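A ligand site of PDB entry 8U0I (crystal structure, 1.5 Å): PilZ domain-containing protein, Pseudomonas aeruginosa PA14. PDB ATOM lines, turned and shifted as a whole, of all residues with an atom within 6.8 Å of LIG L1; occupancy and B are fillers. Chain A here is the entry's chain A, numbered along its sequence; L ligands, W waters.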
ATOM      1  N   ASP A   4      19.910  27.944 -17.333  1.00  0.00           N
ATOM      2  CA  ASP A   4      19.989  27.457 -18.739  1.00  0.00           C
ATOM      3  C   ASP A   4      21.403  27.687 -19.306  1.00  0.00           C
ATOM      4  O   ASP A   4      21.830  26.953 -20.166  1.00  0.00           O
ATOM      5  CB  ASP A   4      18.838  27.919 -19.632  1.00  0.00           C
ATOM      6  CG  ASP A   4      18.509  29.410 -19.775  1.00  0.00           C
ATOM      7  OD1 ASP A   4      19.070  30.261 -19.042  1.00  0.00           O
ATOM      8  OD2 ASP A   4      17.684  29.731 -20.658  1.00  0.00           O
ATOM      9  N   ASN A   5      22.161  28.660 -18.800  1.00  0.00           N
ATOM     10  CA  ASN A   5      23.452  28.985 -19.431  1.00  0.00           C
ATOM     11  C   ASN A   5      24.414  27.837 -19.155  1.00  0.00           C
ATOM     12  O   ASN A   5      24.769  27.594 -18.005  1.00  0.00           O
ATOM     13  CB  ASN A   5      23.980  30.314 -18.907  1.00  0.00           C
ATOM     14  CG  ASN A   5      25.388  30.636 -19.351  1.00  0.00           C
ATOM     15  OD1 ASN A   5      25.880  30.092 -20.348  1.00  0.00           O
ATOM     16  ND2 ASN A   5      26.012  31.544 -18.632  1.00  0.00           N
ATOM     17  N   GLN A   6      24.845  27.124 -20.205  1.00  0.00           N
ATOM     18  CA  GLN A   6      25.750  26.005 -19.998  1.00  0.00           C
ATOM     19  C   GLN A   6      27.229  26.346 -20.194  1.00  0.00           C
ATOM     20  O   GLN A   6      28.103  25.478 -20.046  1.00  0.00           O
ATOM     21  CB  GLN A   6      25.410  24.961 -21.036  1.00  0.00           C
ATOM     22  CG  GLN A   6      23.943  24.596 -21.085  1.00  0.00           C
ATOM     23  CD  GLN A   6      23.604  24.194 -22.496  1.00  0.00           C
ATOM     24  OE1 GLN A   6      23.676  22.991 -22.798  1.00  0.00           O
ATOM     25  NE2 GLN A   6      23.443  25.178 -23.397  1.00  0.00           N
ATOM     26  N   ARG A   7      27.525  27.580 -20.578  1.00  0.00           N
ATOM     27  CA  ARG A   7      28.917  27.985 -20.693  1.00  0.00           C
ATOM     28  C   ARG A   7      29.588  28.254 -19.386  1.00  0.00           C
ATOM     29  O   ARG A   7      29.112  29.108 -18.628  1.00  0.00           O
ATOM     30  CB  ARG A   7      29.040  29.258 -21.541  1.00  0.00           C
ATOM     31  CG  ARG A   7      28.451  29.031 -22.898  1.00  0.00           C
ATOM     32  CD  ARG A   7      28.396  30.325 -23.754  1.00  0.00           C
ATOM     33  NE  ARG A   7      27.675  30.141 -24.989  1.00  0.00           N
ATOM     34  CZ  ARG A   7      27.374  31.025 -25.918  1.00  0.00           C
ATOM     35  NH1 ARG A   7      27.789  32.268 -25.747  1.00  0.00           N
ATOM     36  NH2 ARG A   7      26.718  30.707 -26.992  1.00  0.00           N
ATOM     37  N   PRO A  10      32.259  33.086 -19.991  1.00  0.00           N
ATOM     38  CA  PRO A  10      31.620  33.911 -20.994  1.00  0.00           C
ATOM     39  C   PRO A  10      32.492  34.208 -22.208  1.00  0.00           C
ATOM     40  O   PRO A  10      33.727  34.305 -22.117  1.00  0.00           O
ATOM     41  CB  PRO A  10      31.361  35.207 -20.213  1.00  0.00           C
ATOM     42  CG  PRO A  10      32.466  35.265 -19.233  1.00  0.00           C
ATOM     43  CD  PRO A  10      32.706  33.837 -18.795  1.00  0.00           C
ATOM     44  N   ARG A  11      31.830  34.363 -23.330  1.00  0.00           N
ATOM     45  CA  ARG A  11      32.490  34.627 -24.598  1.00  0.00           C
ATOM     46  C   ARG A  11      32.362  36.094 -24.938  1.00  0.00           C
ATOM     47  O   ARG A  11      31.297  36.642 -24.706  1.00  0.00           O
ATOM     48  CB  ARG A  11      31.900  33.843 -25.758  1.00  0.00           C
ATOM     49  CG  ARG A  11      31.954  32.354 -25.438  1.00  0.00           C
ATOM     50  CD  ARG A  11      31.253  31.544 -26.451  1.00  0.00           C
ATOM     51  NE  ARG A  11      31.229  30.128 -26.056  1.00  0.00           N
ATOM     52  CZ  ARG A  11      30.548  29.214 -26.668  1.00  0.00           C
ATOM     53  NH1 ARG A  11      29.922  29.534 -27.768  1.00  0.00           N
ATOM     54  NH2 ARG A  11      30.526  27.963 -26.234  1.00  0.00           N
ATOM     55  N   ASP A  34      35.206  34.880 -31.567  1.00  0.00           N
ATOM     56  CA  ASP A  34      34.893  35.109 -30.182  1.00  0.00           C
ATOM     57  C   ASP A  34      35.710  34.137 -29.334  1.00  0.00           C
ATOM     58  O   ASP A  34      36.250  33.186 -29.856  1.00  0.00           O
ATOM     59  CB  ASP A  34      33.401  34.977 -29.910  1.00  0.00           C
ATOM     60  CG  ASP A  34      32.818  33.654 -30.284  1.00  0.00           C
ATOM     61  OD1 ASP A  34      33.170  32.661 -29.609  1.00  0.00           O
ATOM     62  OD2 ASP A  34      32.079  33.613 -31.320  1.00  0.00           O
ATOM     63  N   TYR A  41      35.984  30.522 -31.329  1.00  0.00           N
ATOM     64  CA  TYR A  41      35.400  30.219 -32.621  1.00  0.00           C
ATOM     65  C   TYR A  41      36.332  30.801 -33.663  1.00  0.00           C
ATOM     66  O   TYR A  41      36.785  31.954 -33.553  1.00  0.00           O
ATOM     67  CB  TYR A  41      34.011  30.829 -32.707  1.00  0.00           C
ATOM     68  CG  TYR A  41      33.362  30.531 -34.050  1.00  0.00           C
ATOM     69  CD1 TYR A  41      33.693  31.252 -35.189  1.00  0.00           C
ATOM     70  CD2 TYR A  41      32.562  29.421 -34.174  1.00  0.00           C
ATOM     71  CE1 TYR A  41      33.119  30.947 -36.408  1.00  0.00           C
ATOM     72  CE2 TYR A  41      31.957  29.101 -35.378  1.00  0.00           C
ATOM     73  CZ  TYR A  41      32.229  29.894 -36.489  1.00  0.00           C
ATOM     74  OH  TYR A  41      31.641  29.584 -37.682  1.00  0.00           O
ATOM     75  N   VAL A  75      35.377  20.950 -31.495  1.00  0.00           N
ATOM     76  CA  VAL A  75      34.219  20.372 -30.863  1.00  0.00           C
ATOM     77  C   VAL A  75      33.008  20.450 -31.737  1.00  0.00           C
ATOM     78  O   VAL A  75      32.064  19.684 -31.510  1.00  0.00           O
ATOM     79  CB  VAL A  75      33.952  20.979 -29.470  1.00  0.00           C
ATOM     80  CG1 VAL A  75      35.149  20.821 -28.535  1.00  0.00           C
ATOM     81  CG2 VAL A  75      33.500  22.418 -29.556  1.00  0.00           C
ATOM     82  N   ARG A  76      32.988  21.327 -32.744  1.00  0.00           N
ATOM     83  CA  ARG A  76      31.843  21.469 -33.595  1.00  0.00           C
ATOM     84  C   ARG A  76      32.239  22.262 -34.840  1.00  0.00           C
ATOM     85  O   ARG A  76      33.246  22.989 -34.826  1.00  0.00           O
ATOM     86  CB  ARG A  76      30.748  22.213 -32.825  1.00  0.00           C
ATOM     87  CG  ARG A  76      31.038  23.695 -32.626  1.00  0.00           C
ATOM     88  CD  ARG A  76      30.037  24.384 -31.727  1.00  0.00           C
ATOM     89  NE  ARG A  76      30.103  25.846 -31.718  1.00  0.00           N
ATOM     90  CZ  ARG A  76      29.604  26.623 -32.635  1.00  0.00           C
ATOM     91  NH1 ARG A  76      28.919  26.150 -33.656  1.00  0.00           N
ATOM     92  NH2 ARG A  76      29.793  27.917 -32.540  1.00  0.00           N
ATOM     93  N   ASP A  78      30.334  24.497 -38.221  1.00  0.00           N
ATOM     94  CA  ASP A  78      29.102  25.042 -38.766  1.00  0.00           C
ATOM     95  C   ASP A  78      29.393  25.548 -40.168  1.00  0.00           C
ATOM     96  O   ASP A  78      30.428  25.240 -40.717  1.00  0.00           O
ATOM     97  CB  ASP A  78      28.476  25.991 -37.761  1.00  0.00           C
ATOM     98  CG  ASP A  78      29.231  27.279 -37.518  1.00  0.00           C
ATOM     99  OD1 ASP A  78      30.126  27.604 -38.318  1.00  0.00           O
ATOM    100  OD2 ASP A  78      28.909  27.954 -36.521  1.00  0.00           O
HETATM  101  P1  LIG L   1      25.502  32.280 -30.430  1.00  0.00           P
HETATM  102  O1  LIG L   1      26.397  32.352 -29.248  1.00  0.00           O
HETATM  103  O2  LIG L   1      25.706  33.333 -31.511  1.00  0.00           O
HETATM  104  O3  LIG L   1      25.475  30.815 -31.015  1.00  0.00           O
HETATM  105  C1  LIG L   1      24.945  30.519 -32.335  1.00  0.00           C
HETATM  106  C2  LIG L   1      24.797  29.029 -32.508  1.00  0.00           C
HETATM  107  O4  LIG L   1      26.097  28.371 -32.517  1.00  0.00           O
HETATM  108  C3  LIG L   1      24.037  28.287 -31.436  1.00  0.00           C
HETATM  109  O5  LIG L   1      22.649  28.409 -31.692  1.00  0.00           O
HETATM  110  C4  LIG L   1      24.504  26.866 -31.670  1.00  0.00           C
HETATM  111  O6  LIG L   1      23.983  26.324 -32.862  1.00  0.00           O
HETATM  112  C5  LIG L   1      25.980  27.109 -31.918  1.00  0.00           C
HETATM  113  N1  LIG L   1      26.808  27.093 -30.725  1.00  0.00           N
HETATM  114  C6  LIG L   1      27.381  28.140 -30.057  1.00  0.00           C
HETATM  115  N2  LIG L   1      28.101  27.772 -29.034  1.00  0.00           N
HETATM  116  C7  LIG L   1      28.045  26.395 -29.084  1.00  0.00           C
HETATM  117  C8  LIG L   1      28.630  25.473 -28.205  1.00  0.00           C
HETATM  118  O7  LIG L   1      29.411  25.647 -27.279  1.00  0.00           O
HETATM  119  N3  LIG L   1      28.331  24.164 -28.632  1.00  0.00           N
HETATM  120  C9  LIG L   1      27.470  23.841 -29.648  1.00  0.00           C
HETATM  121  N4  LIG L   1      27.293  22.529 -29.858  1.00  0.00           N
HETATM  122  N5  LIG L   1      26.896  24.711 -30.466  1.00  0.00           N
HETATM  123  C10 LIG L   1      27.213  25.969 -30.084  1.00  0.00           C
HETATM  124  P2  LIG L   1      21.701  28.158 -30.447  1.00  0.00           P
HETATM  125  O8  LIG L   1      22.024  26.972 -29.594  1.00  0.00           O
HETATM  126  O9  LIG L   1      20.318  28.159 -31.044  1.00  0.00           O
HETATM  127  O10 LIG L   1      21.822  29.420 -29.475  1.00  0.00           O
HETATM  128  C11 LIG L   1      21.422  30.698 -30.014  1.00  0.00           C
HETATM  129  C12 LIG L   1      21.940  31.758 -29.080  1.00  0.00           C
HETATM  130  O11 LIG L   1      21.483  31.519 -27.753  1.00  0.00           O
HETATM  131  C13 LIG L   1      23.466  31.811 -28.939  1.00  0.00           C
HETATM  132  O12 LIG L   1      23.958  32.563 -30.025  1.00  0.00           O
HETATM  133  C14 LIG L   1      23.601  32.515 -27.604  1.00  0.00           C
HETATM  134  O13 LIG L   1      23.348  33.903 -27.704  1.00  0.00           O
HETATM  135  C15 LIG L   1      22.507  31.782 -26.850  1.00  0.00           C
HETATM  136  N6  LIG L   1      22.900  30.545 -26.186  1.00  0.00           N
HETATM  137  C16 LIG L   1      22.434  29.279 -26.395  1.00  0.00           C
HETATM  138  N7  LIG L   1      22.852  28.443 -25.481  1.00  0.00           N
HETATM  139  C17 LIG L   1      23.617  29.205 -24.621  1.00  0.00           C
HETATM  140  C18 LIG L   1      24.280  28.894 -23.436  1.00  0.00           C
HETATM  141  O14 LIG L   1      24.400  27.800 -22.860  1.00  0.00           O
HETATM  142  N8  LIG L   1      24.895  30.006 -22.863  1.00  0.00           N
HETATM  143  C19 LIG L   1      24.802  31.302 -23.344  1.00  0.00           C
HETATM  144  N9  LIG L   1      25.503  32.239 -22.691  1.00  0.00           N
HETATM  145  N10 LIG L   1      24.235  31.573 -24.492  1.00  0.00           N
HETATM  146  C20 LIG L   1      23.613  30.522 -25.037  1.00  0.00           C
HETATM  147  P1  LG2 L   2      30.619  21.790 -26.474  1.00  0.00           P
HETATM  148  O1  LG2 L   2      31.283  20.439 -26.273  1.00  0.00           O
HETATM  149  O2  LG2 L   2      29.753  22.063 -27.626  1.00  0.00           O
HETATM  150  O3  LG2 L   2      31.787  22.886 -26.380  1.00  0.00           O
HETATM  151  C1  LG2 L   2      32.844  22.737 -25.484  1.00  0.00           C
HETATM  152  C2  LG2 L   2      33.638  24.008 -25.402  1.00  0.00           C
HETATM  153  O4  LG2 L   2      34.137  24.385 -26.710  1.00  0.00           O
HETATM  154  C3  LG2 L   2      32.875  25.242 -24.948  1.00  0.00           C
HETATM  155  O5  LG2 L   2      32.644  25.162 -23.560  1.00  0.00           O
HETATM  156  C4  LG2 L   2      33.901  26.275 -25.317  1.00  0.00           C
HETATM  157  O6  LG2 L   2      35.042  26.337 -24.503  1.00  0.00           O
HETATM  158  C5  LG2 L   2      34.257  25.795 -26.721  1.00  0.00           C
HETATM  159  N1  LG2 L   2      33.433  26.318 -27.800  1.00  0.00           N
HETATM  160  C6  LG2 L   2      32.495  25.680 -28.577  1.00  0.00           C
HETATM  161  N2  LG2 L   2      31.937  26.444 -29.489  1.00  0.00           N
HETATM  162  C7  LG2 L   2      32.525  27.680 -29.231  1.00  0.00           C
HETATM  163  C8  LG2 L   2      32.283  28.946 -29.842  1.00  0.00           C
HETATM  164  O7  LG2 L   2      31.543  29.203 -30.792  1.00  0.00           O
HETATM  165  N3  LG2 L   2      33.067  29.927 -29.253  1.00  0.00           N
HETATM  166  C9  LG2 L   2      33.949  29.767 -28.216  1.00  0.00           C
HETATM  167  N4  LG2 L   2      34.558  30.866 -27.782  1.00  0.00           N
HETATM  168  N5  LG2 L   2      34.162  28.605 -27.620  1.00  0.00           N
HETATM  169  C10 LG2 L   2      33.403  27.627 -28.177  1.00  0.00           C
HETATM  170  P2  LG2 L   2      31.459  26.024 -22.892  1.00  0.00           P
HETATM  171  O8  LG2 L   2      31.398  27.351 -23.616  1.00  0.00           O
HETATM  172  O9  LG2 L   2      31.709  25.903 -21.421  1.00  0.00           O
HETATM  173  O10 LG2 L   2      30.145  25.310 -23.405  1.00  0.00           O
HETATM  174  C11 LG2 L   2      29.895  23.995 -22.751  1.00  0.00           C
HETATM  175  C12 LG2 L   2      28.799  23.292 -23.485  1.00  0.00           C
HETATM  176  O11 LG2 L   2      27.566  24.035 -23.350  1.00  0.00           O
HETATM  177  C13 LG2 L   2      28.979  23.092 -24.978  1.00  0.00           C
HETATM  178  O12 LG2 L   2      29.847  21.944 -25.094  1.00  0.00           O
HETATM  179  C14 LG2 L   2      27.523  22.856 -25.400  1.00  0.00           C
HETATM  180  O13 LG2 L   2      27.077  21.544 -25.080  1.00  0.00           O
HETATM  181  C15 LG2 L   2      26.822  23.872 -24.528  1.00  0.00           C
HETATM  182  N6  LG2 L   2      26.692  25.171 -25.172  1.00  0.00           N
HETATM  183  C16 LG2 L   2      27.285  26.359 -24.817  1.00  0.00           C
HETATM  184  N7  LG2 L   2      26.896  27.343 -25.576  1.00  0.00           N
HETATM  185  C17 LG2 L   2      25.950  26.803 -26.425  1.00  0.00           C
HETATM  186  C18 LG2 L   2      25.156  27.386 -27.450  1.00  0.00           C
HETATM  187  O14 LG2 L   2      25.127  28.560 -27.849  1.00  0.00           O
HETATM  188  N8  LG2 L   2      24.290  26.454 -28.039  1.00  0.00           N
HETATM  189  C19 LG2 L   2      24.277  25.112 -27.742  1.00  0.00           C
HETATM  190  N9  LG2 L   2      23.413  24.346 -28.430  1.00  0.00           N
HETATM  191  N10 LG2 L   2      25.034  24.570 -26.804  1.00  0.00           N
HETATM  192  C20 LG2 L   2      25.833  25.457 -26.185  1.00  0.00           C
HETATM  193  O   HOH W   1      26.941  21.376 -32.808  1.00  0.00           O
HETATM  194  O   HOH W   2      28.329  29.494 -34.384  1.00  0.00           O
HETATM  195  O   HOH W   3      21.913  25.965 -25.327  1.00  0.00           O
HETATM  196  O   HOH W   4      24.770  35.263 -25.936  1.00  0.00           O
HETATM  197  O   HOH W   5      20.316  26.031 -27.617  1.00  0.00           O
HETATM  198  O   HOH W   6      29.242  32.028 -29.144  1.00  0.00           O
HETATM  199  O   HOH W   7      29.533  20.157 -29.449  1.00  0.00           O
HETATM  200  O   HOH W   8      26.913  34.363 -27.403  1.00  0.00           O
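O of Asp 4 touches O14 of LIG L1 (3.8 Å). Arg 76 touches LIG L1. Six residues have an atom within 4 Å of LIG L1: Asp 4, Asn 5, Gln 6, Arg 7, Arg 11 and Arg 76. Along chain A the residues within 4 Å of LIG L1 span positions 4 to 76. The nearest printed residue that does not touch LIG L1 is Asp 78 (4.9 Å).
Water W3 lies within hydrogen-bond range of the side-chain amide nitrogen of Gln 6 (2.6 Å) and a nitrogen (N7) of LIG L1 (2.7 Å). Water W8 lies within hydrogen-bond range of O1 of LIG L1 (2.8 Å) and NH1 of Arg 7 (2.8 Å). Water W6 bridges O1 of LIG L1 (2.9 Å) and NH1 of Arg 11 (2.9 Å). Water W2 lies within hydrogen-bond range of the side-chain carboxylate (OD2) of Asp 78, the guanidinium group (NH2) of Arg 76 and an oxygen (O4) of LIG L1. Water W7 lies within hydrogen-bond range of an oxygen (O2) of LG2 L2, a nitrogen (N4) of LIG L1 and the backbone carbonyl oxygen of Val 75.
NH2 of Arg 11 lies within salt-bridge range of O8 of LG2 L2 (2.8 Å). An oxygen (O7) of LIG L1 lies within hydrogen-bond range of the guanidinium group (NH2) of Arg 11, at 2.8 Å. O1 of LIG L1 is in salt-bridge range of NH2 of Arg 7, at 2.8 Å. A nitrogen (N3) of LG2 L2 lies within hydrogen-bond range of the side-chain carboxylate (OD1) of Asp 34, at 2.8 Å. OD1 of Asn 5 lies within hydrogen-bond range of N8 of LIG L1, 2.7 Å away. NE2 of Gln 6 lies within hydrogen-bond range of O14 of LIG L1 (2.8 Å). The guanidinium group (NH2) of Arg 76 sits at hydrogen-bond distance from an oxygen (O7) of LG2 L2. An oxygen (O14) of LIG L1 is in hydrogen-bond range of the backbone NH (N) of Gln 6 (2.8 Å). NH2 of Arg 7 sits at hydrogen-bond distance from O14 of LG2 L2 (2.8 Å).
N of Arg 7 is in hydrogen-bond range of OD1 of Asn 5 (3.0 Å). The guanidinium group (NH1) of Arg 76 lies within salt-bridge range of the side-chain carboxylate (OD2) of Asp 78, 3.4 Å away.
O2 of LG2 L2 is in hydrogen-bond range of N3 of LIG L1.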
